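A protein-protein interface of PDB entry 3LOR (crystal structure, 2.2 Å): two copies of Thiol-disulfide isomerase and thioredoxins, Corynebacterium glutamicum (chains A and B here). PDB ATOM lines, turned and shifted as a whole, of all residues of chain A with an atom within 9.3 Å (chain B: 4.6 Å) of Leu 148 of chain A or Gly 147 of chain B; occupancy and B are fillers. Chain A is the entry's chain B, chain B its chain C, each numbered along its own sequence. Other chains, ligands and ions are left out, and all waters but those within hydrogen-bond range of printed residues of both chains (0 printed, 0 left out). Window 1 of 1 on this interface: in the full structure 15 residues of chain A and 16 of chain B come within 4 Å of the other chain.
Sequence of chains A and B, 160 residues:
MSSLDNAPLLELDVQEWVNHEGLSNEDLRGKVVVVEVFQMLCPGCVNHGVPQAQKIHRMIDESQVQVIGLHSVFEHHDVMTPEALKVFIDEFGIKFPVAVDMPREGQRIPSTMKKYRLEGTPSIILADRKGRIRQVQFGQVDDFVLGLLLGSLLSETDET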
ATOM      1  N   ILE A  60     -33.864   5.790 -26.640  1.00  0.00           N
ATOM      2  CA  ILE A  60     -33.284   6.820 -25.868  1.00  0.00           C
ATOM      3  C   ILE A  60     -33.593   8.095 -26.570  1.00  0.00           C
ATOM      4  O   ILE A  60     -33.388   8.225 -27.726  1.00  0.00           O
ATOM      5  CB  ILE A  60     -31.806   6.618 -25.768  1.00  0.00           C
ATOM      6  CG1 ILE A  60     -31.528   5.210 -25.326  1.00  0.00           C
ATOM      7  CG2 ILE A  60     -31.226   7.590 -24.835  1.00  0.00           C
ATOM      8  CD1 ILE A  60     -30.158   4.954 -24.979  1.00  0.00           C
ATOM      9  N   LEU A 126     -18.299   6.412 -30.416  1.00  0.00           N
ATOM     10  CA  LEU A 126     -19.021   7.036 -29.333  1.00  0.00           C
ATOM     11  C   LEU A 126     -18.298   8.235 -28.816  1.00  0.00           C
ATOM     12  O   LEU A 126     -17.145   8.172 -28.554  1.00  0.00           O
ATOM     13  CB  LEU A 126     -19.264   6.087 -28.183  1.00  0.00           C
ATOM     14  CG  LEU A 126     -19.899   4.723 -28.373  1.00  0.00           C
ATOM     15  CD1 LEU A 126     -19.994   4.011 -27.116  1.00  0.00           C
ATOM     16  CD2 LEU A 126     -21.196   4.754 -29.085  1.00  0.00           C
ATOM     17  N   GLN A 135     -14.848   5.902 -27.539  1.00  0.00           N
ATOM     18  CA  GLN A 135     -14.691   4.572 -28.033  1.00  0.00           C
ATOM     19  C   GLN A 135     -14.827   4.509 -29.522  1.00  0.00           C
ATOM     20  O   GLN A 135     -15.571   5.234 -30.092  1.00  0.00           O
ATOM     21  CB  GLN A 135     -15.720   3.639 -27.421  1.00  0.00           C
ATOM     22  CG  GLN A 135     -15.337   3.068 -26.144  1.00  0.00           C
ATOM     23  CD  GLN A 135     -14.516   1.833 -26.290  1.00  0.00           C
ATOM     24  OE1 GLN A 135     -14.715   1.030 -27.179  1.00  0.00           O
ATOM     25  NE2 GLN A 135     -13.588   1.677 -25.408  1.00  0.00           N
ATOM     26  N   VAL A 141     -21.006  -5.622 -32.181  1.00  0.00           N
ATOM     27  CA  VAL A 141     -20.967  -5.267 -30.776  1.00  0.00           C
ATOM     28  C   VAL A 141     -22.188  -5.791 -30.057  1.00  0.00           C
ATOM     29  O   VAL A 141     -23.269  -5.587 -30.478  1.00  0.00           O
ATOM     30  CB  VAL A 141     -20.934  -3.776 -30.542  1.00  0.00           C
ATOM     31  CG1 VAL A 141     -20.591  -3.502 -29.151  1.00  0.00           C
ATOM     32  CG2 VAL A 141     -19.982  -3.094 -31.448  1.00  0.00           C
ATOM     33  N   ASP A 142     -21.976  -6.455 -28.947  1.00  0.00           N
ATOM     34  CA  ASP A 142     -23.042  -7.008 -28.142  1.00  0.00           C
ATOM     35  C   ASP A 142     -23.916  -5.890 -27.587  1.00  0.00           C
ATOM     36  O   ASP A 142     -23.435  -4.874 -27.214  1.00  0.00           O
ATOM     37  CB  ASP A 142     -22.410  -7.809 -27.011  1.00  0.00           C
ATOM     38  CG  ASP A 142     -23.328  -8.830 -26.414  1.00  0.00           C
ATOM     39  OD1 ASP A 142     -23.204  -9.998 -26.737  1.00  0.00           O
ATOM     40  OD2 ASP A 142     -24.169  -8.475 -25.603  1.00  0.00           O
ATOM     41  N   ASP A 143     -25.205  -6.112 -27.518  1.00  0.00           N
ATOM     42  CA  ASP A 143     -26.121  -5.122 -27.000  1.00  0.00           C
ATOM     43  C   ASP A 143     -25.798  -4.775 -25.565  1.00  0.00           C
ATOM     44  O   ASP A 143     -25.908  -3.660 -25.192  1.00  0.00           O
ATOM     45  CB  ASP A 143     -27.545  -5.650 -27.013  1.00  0.00           C
ATOM     46  CG  ASP A 143     -28.286  -5.390 -28.302  1.00  0.00           C
ATOM     47  OD1 ASP A 143     -27.876  -4.560 -29.081  1.00  0.00           O
ATOM     48  OD2 ASP A 143     -29.327  -6.010 -28.511  1.00  0.00           O
ATOM     49  N   PHE A 144     -25.428  -5.756 -24.769  1.00  0.00           N
ATOM     50  CA  PHE A 144     -25.104  -5.508 -23.391  1.00  0.00           C
ATOM     51  C   PHE A 144     -23.915  -4.616 -23.198  1.00  0.00           C
ATOM     52  O   PHE A 144     -23.959  -3.732 -22.411  1.00  0.00           O
ATOM     53  CB  PHE A 144     -24.856  -6.805 -22.631  1.00  0.00           C
ATOM     54  CG  PHE A 144     -24.436  -6.588 -21.243  1.00  0.00           C
ATOM     55  CD1 PHE A 144     -25.296  -6.103 -20.334  1.00  0.00           C
ATOM     56  CD2 PHE A 144     -23.169  -6.821 -20.854  1.00  0.00           C
ATOM     57  CE1 PHE A 144     -24.912  -5.890 -19.072  1.00  0.00           C
ATOM     58  CE2 PHE A 144     -22.785  -6.601 -19.570  1.00  0.00           C
ATOM     59  CZ  PHE A 144     -23.659  -6.135 -18.688  1.00  0.00           C
ATOM     60  N   VAL A 145     -22.865  -4.870 -23.951  1.00  0.00           N
ATOM     61  CA  VAL A 145     -21.673  -4.068 -23.940  1.00  0.00           C
ATOM     62  C   VAL A 145     -21.974  -2.673 -24.390  1.00  0.00           C
ATOM     63  O   VAL A 145     -21.515  -1.747 -23.806  1.00  0.00           O
ATOM     64  CB  VAL A 145     -20.607  -4.627 -24.869  1.00  0.00           C
ATOM     65  CG1 VAL A 145     -19.512  -3.665 -25.027  1.00  0.00           C
ATOM     66  CG2 VAL A 145     -20.120  -5.909 -24.381  1.00  0.00           C
ATOM     67  N   LEU A 146     -22.781  -2.535 -25.416  1.00  0.00           N
ATOM     68  CA  LEU A 146     -23.134  -1.222 -25.885  1.00  0.00           C
ATOM     69  C   LEU A 146     -23.868  -0.391 -24.865  1.00  0.00           C
ATOM     70  O   LEU A 146     -23.591   0.746 -24.709  1.00  0.00           O
ATOM     71  CB  LEU A 146     -23.950  -1.310 -27.148  1.00  0.00           C
ATOM     72  CG  LEU A 146     -24.222  -0.064 -27.955  1.00  0.00           C
ATOM     73  CD1 LEU A 146     -23.052   0.823 -28.126  1.00  0.00           C
ATOM     74  CD2 LEU A 146     -24.773  -0.433 -29.258  1.00  0.00           C
ATOM     75  N   GLY A 147     -24.792  -0.999 -24.157  1.00  0.00           N
ATOM     76  CA  GLY A 147     -25.499  -0.338 -23.103  1.00  0.00           C
ATOM     77  C   GLY A 147     -24.610   0.079 -21.974  1.00  0.00           C
ATOM     78  O   GLY A 147     -24.742   1.135 -21.481  1.00  0.00           O
ATOM     79  N   LEU A 148     -23.686  -0.764 -21.586  1.00  0.00           N
ATOM     80  CA  LEU A 148     -22.810  -0.415 -20.517  1.00  0.00           C
ATOM     81  C   LEU A 148     -22.013   0.821 -20.891  1.00  0.00           C
ATOM     82  O   LEU A 148     -21.907   1.724 -20.118  1.00  0.00           O
ATOM     83  CB  LEU A 148     -21.864  -1.548 -20.217  1.00  0.00           C
ATOM     84  CG  LEU A 148     -22.175  -2.523 -19.102  1.00  0.00           C
ATOM     85  CD1 LEU A 148     -21.301  -3.698 -19.214  1.00  0.00           C
ATOM     86  CD2 LEU A 148     -22.091  -1.904 -17.759  1.00  0.00           C
ATOM     87  N   LEU A 149     -21.517   0.870 -22.112  1.00  0.00           N
ATOM     88  CA  LEU A 149     -20.756   2.000 -22.565  1.00  0.00           C
ATOM     89  C   LEU A 149     -21.545   3.285 -22.594  1.00  0.00           C
ATOM     90  O   LEU A 149     -21.069   4.270 -22.138  1.00  0.00           O
ATOM     91  CB  LEU A 149     -20.169   1.729 -23.940  1.00  0.00           C
ATOM     92  CG  LEU A 149     -19.205   0.574 -24.085  1.00  0.00           C
ATOM     93  CD1 LEU A 149     -18.938   0.196 -25.455  1.00  0.00           C
ATOM     94  CD2 LEU A 149     -17.975   0.897 -23.433  1.00  0.00           C
ATOM     95  N   LEU A 150     -22.742   3.263 -23.140  1.00  0.00           N
ATOM     96  CA  LEU A 150     -23.590   4.423 -23.172  1.00  0.00           C
ATOM     97  C   LEU A 150     -24.070   4.890 -21.804  1.00  0.00           C
ATOM     98  O   LEU A 150     -24.111   6.041 -21.543  1.00  0.00           O
ATOM     99  CB  LEU A 150     -24.768   4.199 -24.096  1.00  0.00           C
ATOM    100  CG  LEU A 150     -24.538   4.118 -25.590  1.00  0.00           C
ATOM    101  CD1 LEU A 150     -25.768   3.695 -26.223  1.00  0.00           C
ATOM    102  CD2 LEU A 150     -24.147   5.426 -26.130  1.00  0.00           C
ATOM    103  N   GLY A 151     -24.466   3.965 -20.963  1.00  0.00           N
ATOM    104  CA  GLY A 151     -24.965   4.307 -19.658  1.00  0.00           C
ATOM    105  C   GLY A 151     -23.882   4.984 -18.889  1.00  0.00           C
ATOM    106  O   GLY A 151     -24.095   5.951 -18.252  1.00  0.00           O
ATOM    107  N   SER A 152     -22.692   4.464 -19.048  1.00  0.00           N
ATOM    108  CA  SER A 152     -21.530   5.015 -18.440  1.00  0.00           C
ATOM    109  C   SER A 152     -21.247   6.426 -18.896  1.00  0.00           C
ATOM    110  O   SER A 152     -21.087   7.286 -18.092  1.00  0.00           O
ATOM    111  CB  SER A 152     -20.373   4.123 -18.792  1.00  0.00           C
ATOM    112  OG  SER A 152     -19.291   4.458 -18.009  1.00  0.00           O
ATOM    113  N   LEU A 153     -21.277   6.667 -20.185  1.00  0.00           N
ATOM    114  CA  LEU A 153     -21.144   7.993 -20.735  1.00  0.00           C
ATOM    115  C   LEU A 153     -22.252   8.935 -20.337  1.00  0.00           C
ATOM    116  O   LEU A 153     -22.016  10.077 -20.139  1.00  0.00           O
ATOM    117  CB  LEU A 153     -20.992   7.950 -22.256  1.00  0.00           C
ATOM    118  CG  LEU A 153     -19.689   7.369 -22.809  1.00  0.00           C
ATOM    119  CD1 LEU A 153     -19.681   6.997 -24.236  1.00  0.00           C
ATOM    120  CD2 LEU A 153     -18.469   8.123 -22.427  1.00  0.00           C
ATOM    121  N   LEU A 154     -23.467   8.452 -20.250  1.00  0.00           N
ATOM    122  CA  LEU A 154     -24.600   9.275 -19.863  1.00  0.00           C
ATOM    123  C   LEU A 154     -24.554   9.804 -18.427  1.00  0.00           C
ATOM    124  O   LEU A 154     -25.026  10.851 -18.155  1.00  0.00           O
ATOM    125  CB  LEU A 154     -25.928   8.631 -20.201  1.00  0.00           C
ATOM    126  CG  LEU A 154     -26.352   8.670 -21.668  1.00  0.00           C
ATOM    127  CD1 LEU A 154     -27.334   7.625 -21.947  1.00  0.00           C
ATOM    128  CD2 LEU A 154     -26.854   9.969 -22.074  1.00  0.00           C
ATOM    129  N   SER A 155     -23.956   9.068 -17.529  1.00  0.00           N
ATOM    130  CA  SER A 155     -23.970   9.442 -16.129  1.00  0.00           C
ATOM    131  C   SER A 155     -22.719  10.169 -15.602  1.00  0.00           C
ATOM    132  O   SER A 155     -22.708  10.649 -14.509  1.00  0.00           O
ATOM    133  CB  SER A 155     -24.300   8.220 -15.290  1.00  0.00           C
ATOM    134  OG  SER A 155     -23.257   7.296 -15.352  1.00  0.00           O
ATOM    135  N   GLU A 156     -21.677  10.223 -16.413  1.00  0.00           N
ATOM    136  CA  GLU A 156     -20.452  10.951 -16.116  1.00  0.00           C
ATOM    137  C   GLU A 156     -20.771  12.372 -15.831  1.00  0.00           C
ATOM    138  O   GLU A 156     -21.510  12.991 -16.538  1.00  0.00           O
ATOM    139  CB  GLU A 156     -19.507  10.927 -17.294  1.00  0.00           C
ATOM    140  CG  GLU A 156     -18.567   9.796 -17.312  1.00  0.00           C
ATOM    141  CD  GLU A 156     -17.596   9.866 -18.455  1.00  0.00           C
ATOM    142  OE1 GLU A 156     -17.615  10.833 -19.206  1.00  0.00           O
ATOM    143  OE2 GLU A 156     -16.821   8.941 -18.619  1.00  0.00           O
ATOM    144  N   ILE B  60     -17.287  -8.604 -16.655  1.00  0.00           N
ATOM    145  CA  ILE B  60     -16.801  -7.519 -15.826  1.00  0.00           C
ATOM    146  C   ILE B  60     -16.206  -8.094 -14.573  1.00  0.00           C
ATOM    147  O   ILE B  60     -16.667  -9.089 -14.085  1.00  0.00           O
ATOM    148  CB  ILE B  60     -17.902  -6.549 -15.440  1.00  0.00           C
ATOM    149  CG1 ILE B  60     -18.437  -5.841 -16.643  1.00  0.00           C
ATOM    150  CG2 ILE B  60     -17.396  -5.493 -14.589  1.00  0.00           C
ATOM    151  CD1 ILE B  60     -19.786  -5.338 -16.410  1.00  0.00           C
ATOM    152  N   ASP B 143     -31.010  -6.984 -22.664  1.00  0.00           N
ATOM    153  CA  ASP B 143     -29.583  -6.940 -22.441  1.00  0.00           C
ATOM    154  C   ASP B 143     -29.131  -5.498 -22.552  1.00  0.00           C
ATOM    155  O   ASP B 143     -28.341  -5.057 -21.789  1.00  0.00           O
ATOM    156  CB  ASP B 143     -28.855  -7.719 -23.519  1.00  0.00           C
ATOM    157  CG  ASP B 143     -28.585  -9.162 -23.163  1.00  0.00           C
ATOM    158  OD1 ASP B 143     -28.751  -9.573 -22.046  1.00  0.00           O
ATOM    159  OD2 ASP B 143     -28.156  -9.891 -24.034  1.00  0.00           O
ATOM    160  N   PHE B 144     -29.667  -4.778 -23.513  1.00  0.00           N
ATOM    161  CA  PHE B 144     -29.340  -3.399 -23.690  1.00  0.00           C
ATOM    162  C   PHE B 144     -29.739  -2.516 -22.519  1.00  0.00           C
ATOM    163  O   PHE B 144     -28.964  -1.753 -22.063  1.00  0.00           O
ATOM    164  CB  PHE B 144     -29.990  -2.899 -24.973  1.00  0.00           C
ATOM    165  CG  PHE B 144     -29.662  -1.498 -25.309  1.00  0.00           C
ATOM    166  CD1 PHE B 144     -28.375  -1.112 -25.504  1.00  0.00           C
ATOM    167  CD2 PHE B 144     -30.636  -0.562 -25.410  1.00  0.00           C
ATOM    168  CE1 PHE B 144     -28.087   0.162 -25.790  1.00  0.00           C
ATOM    169  CE2 PHE B 144     -30.335   0.711 -25.705  1.00  0.00           C
ATOM    170  CZ  PHE B 144     -29.061   1.072 -25.903  1.00  0.00           C
ATOM    171  N   VAL B 145     -30.953  -2.666 -22.042  1.00  0.00           N
ATOM    172  CA  VAL B 145     -31.439  -1.918 -20.925  1.00  0.00           C
ATOM    173  C   VAL B 145     -30.621  -2.220 -19.693  1.00  0.00           C
ATOM    174  O   VAL B 145     -30.274  -1.343 -18.982  1.00  0.00           O
ATOM    175  CB  VAL B 145     -32.896  -2.249 -20.669  1.00  0.00           C
ATOM    176  CG1 VAL B 145     -33.329  -1.715 -19.412  1.00  0.00           C
ATOM    177  CG2 VAL B 145     -33.752  -1.750 -21.791  1.00  0.00           C
ATOM    178  N   LEU B 146     -30.288  -3.471 -19.472  1.00  0.00           N
ATOM    179  CA  LEU B 146     -29.433  -3.849 -18.360  1.00  0.00           C
ATOM    180  C   LEU B 146     -28.017  -3.283 -18.401  1.00  0.00           C
ATOM    181  O   LEU B 146     -27.484  -2.894 -17.414  1.00  0.00           O
ATOM    182  CB  LEU B 146     -29.363  -5.348 -18.185  1.00  0.00           C
ATOM    183  CG  LEU B 146     -28.772  -5.800 -16.854  1.00  0.00           C
ATOM    184  CD1 LEU B 146     -29.365  -5.114 -15.707  1.00  0.00           C
ATOM    185  CD2 LEU B 146     -28.830  -7.248 -16.684  1.00  0.00           C
ATOM    186  N   GLY B 147     -27.430  -3.237 -19.568  1.00  0.00           N
ATOM    187  CA  GLY B 147     -26.168  -2.582 -19.720  1.00  0.00           C
ATOM    188  C   GLY B 147     -26.197  -1.113 -19.394  1.00  0.00           C
ATOM    189  O   GLY B 147     -25.344  -0.642 -18.723  1.00  0.00           O
ATOM    190  N   LEU B 148     -27.204  -0.402 -19.854  1.00  0.00           N
ATOM    191  CA  LEU B 148     -27.327   0.987 -19.547  1.00  0.00           C
ATOM    192  C   LEU B 148     -27.450   1.184 -18.070  1.00  0.00           C
ATOM    193  O   LEU B 148     -26.863   2.075 -17.543  1.00  0.00           O
ATOM    194  CB  LEU B 148     -28.559   1.593 -20.196  1.00  0.00           C
ATOM    195  CG  LEU B 148     -28.654   1.846 -21.687  1.00  0.00           C
ATOM    196  CD1 LEU B 148     -30.035   2.130 -22.085  1.00  0.00           C
ATOM    197  CD2 LEU B 148     -27.744   2.920 -22.143  1.00  0.00           C
ATOM    198  N   LEU B 149     -28.239   0.363 -17.400  1.00  0.00           N
ATOM    199  CA  LEU B 149     -28.410   0.516 -15.974  1.00  0.00           C
ATOM    200  C   LEU B 149     -27.138   0.272 -15.197  1.00  0.00           C
ATOM    201  O   LEU B 149     -26.800   1.028 -14.348  1.00  0.00           O
ATOM    202  CB  LEU B 149     -29.487  -0.392 -15.456  1.00  0.00           C
ATOM    203  CG  LEU B 149     -30.929  -0.131 -15.791  1.00  0.00           C
ATOM    204  CD1 LEU B 149     -31.730  -1.253 -15.292  1.00  0.00           C
ATOM    205  CD2 LEU B 149     -31.374   1.131 -15.232  1.00  0.00           C
ATOM    206  N   LEU B 150     -26.425  -0.776 -15.519  1.00  0.00           N
ATOM    207  CA  LEU B 150     -25.185  -1.015 -14.856  1.00  0.00           C
ATOM    208  C   LEU B 150     -24.182   0.119 -15.115  1.00  0.00           C
ATOM    209  O   LEU B 150     -23.561   0.614 -14.214  1.00  0.00           O
ATOM    210  CB  LEU B 150     -24.609  -2.344 -15.280  1.00  0.00           C
ATOM    211  CG  LEU B 150     -24.969  -3.504 -14.399  1.00  0.00           C
ATOM    212  CD1 LEU B 150     -24.725  -4.765 -15.072  1.00  0.00           C
ATOM    213  CD2 LEU B 150     -24.160  -3.436 -13.165  1.00  0.00           C
ATOM    214  N   GLY B 151     -24.072   0.541 -16.347  1.00  0.00           N
ATOM    215  CA  GLY B 151     -23.116   1.541 -16.720  1.00  0.00           C
ATOM    216  C   GLY B 151     -23.362   2.831 -16.026  1.00  0.00           C
ATOM    217  O   GLY B 151     -22.463   3.497 -15.624  1.00  0.00           O
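Of the 19 printed residues of chain A, 8 touch a printed residue of chain B.
Among the printed residues, no Asp or Glu carboxylate lies within 4 Å of a Lys or Arg side-chain nitrogen of the other chain.
Phe 144 of chain A touches Asp 143 of chain B.
CA of Gly 147 of chain B touches CE1 of Phe 144 of chain A, at 3.6 Å.
CE1 of Phe 144 of chain B touches CA of Gly 147 of chain A, at 3.8 Å.
Leu 148 of chain A touches Ile 60 of chain B.
N of Leu 148 of chain A touches N of Leu 148 of chain B, at 3.9 Å.
CD2 of Leu 148 of chain A touches CB of Leu 150 of chain B, 3.6 Å away.
Leu 148 of chain B touches Leu 150 of chain A.
Gly 151 of chain A touches Leu 148 of chain B.
Ser 152 of chain A touches Gly 151 of chain B.
O of Gly 151 of chain B touches OG of Ser 155 of chain A (3.9 Å).
The backbone NH of Phe 144 of chain A sits at hydrogen-bond distance from the side-chain carboxylate of Asp 142 of chain A (3.1 Å).
O of Gly 151 of chain A sits at hydrogen-bond distance from OG of Ser 155 of chain A (3.3 Å).
The backbone carbonyl oxygen of Ser 152 of chain A lies within hydrogen-bond range of the side-chain hydroxyl of Ser 155 of chain A (3.5 Å).
Asp 143 of chain A touches Phe 144 of chain B, and with the chains exchanged Phe 144 of chain A touches Asp 143 of chain B.
Phe 144 of chain A touches Gly 147 of chain B, and with the chains exchanged Gly 147 of chain A touches Phe 144 of chain B.
Gly 147 of chain B touches its own counterpart, Gly 147 of chain A.
Gly 151 of chain A touches its own counterpart, Gly 151 of chain B.
Positions printed for both chains: 60, 143, 144, 145, 146, 147, 148, 149, 150 and 151.
Of the 16 pairs that touch across the chains among the printed residues, 13 have their exchanged pair printed and touching as well.
The backbone carbonyl oxygen (O) of Gly 147 of chain A sits close to the backbone NH (N) of Leu 148 of chain B (3.3 Å).
The backbone NH (N) of Leu 148 of chain A sits close to the backbone carbonyl oxygen (O) of Gly 147 of chain B, at 3.3 Å.
The backbone carbonyl oxygen (O) of Gly 147 of chain A lies close to the backbone carbonyl oxygen (O) of Gly 147 of chain B, at 3.3 Å.
Printed residues of chain B within 4 Å of Leu 148 of chain A: Ile 60, Gly 147, Leu 148, Leu 150 and Gly 151.
Gly 147 of chain B touches three residues of chain A.
No residue of chain A comes within 4 Å of Leu 146 of chain B.
Gly 151 of chain B touches just these residues of chain A: Leu 148, Gly 151, Ser 152 and Ser 155.
Of the printed residues of chain A, Asp 143 of chain B touches Phe 144.
Of the printed residues of chain B, Gly 147 of chain A touches Phe 144, Gly 147 and Leu 148.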
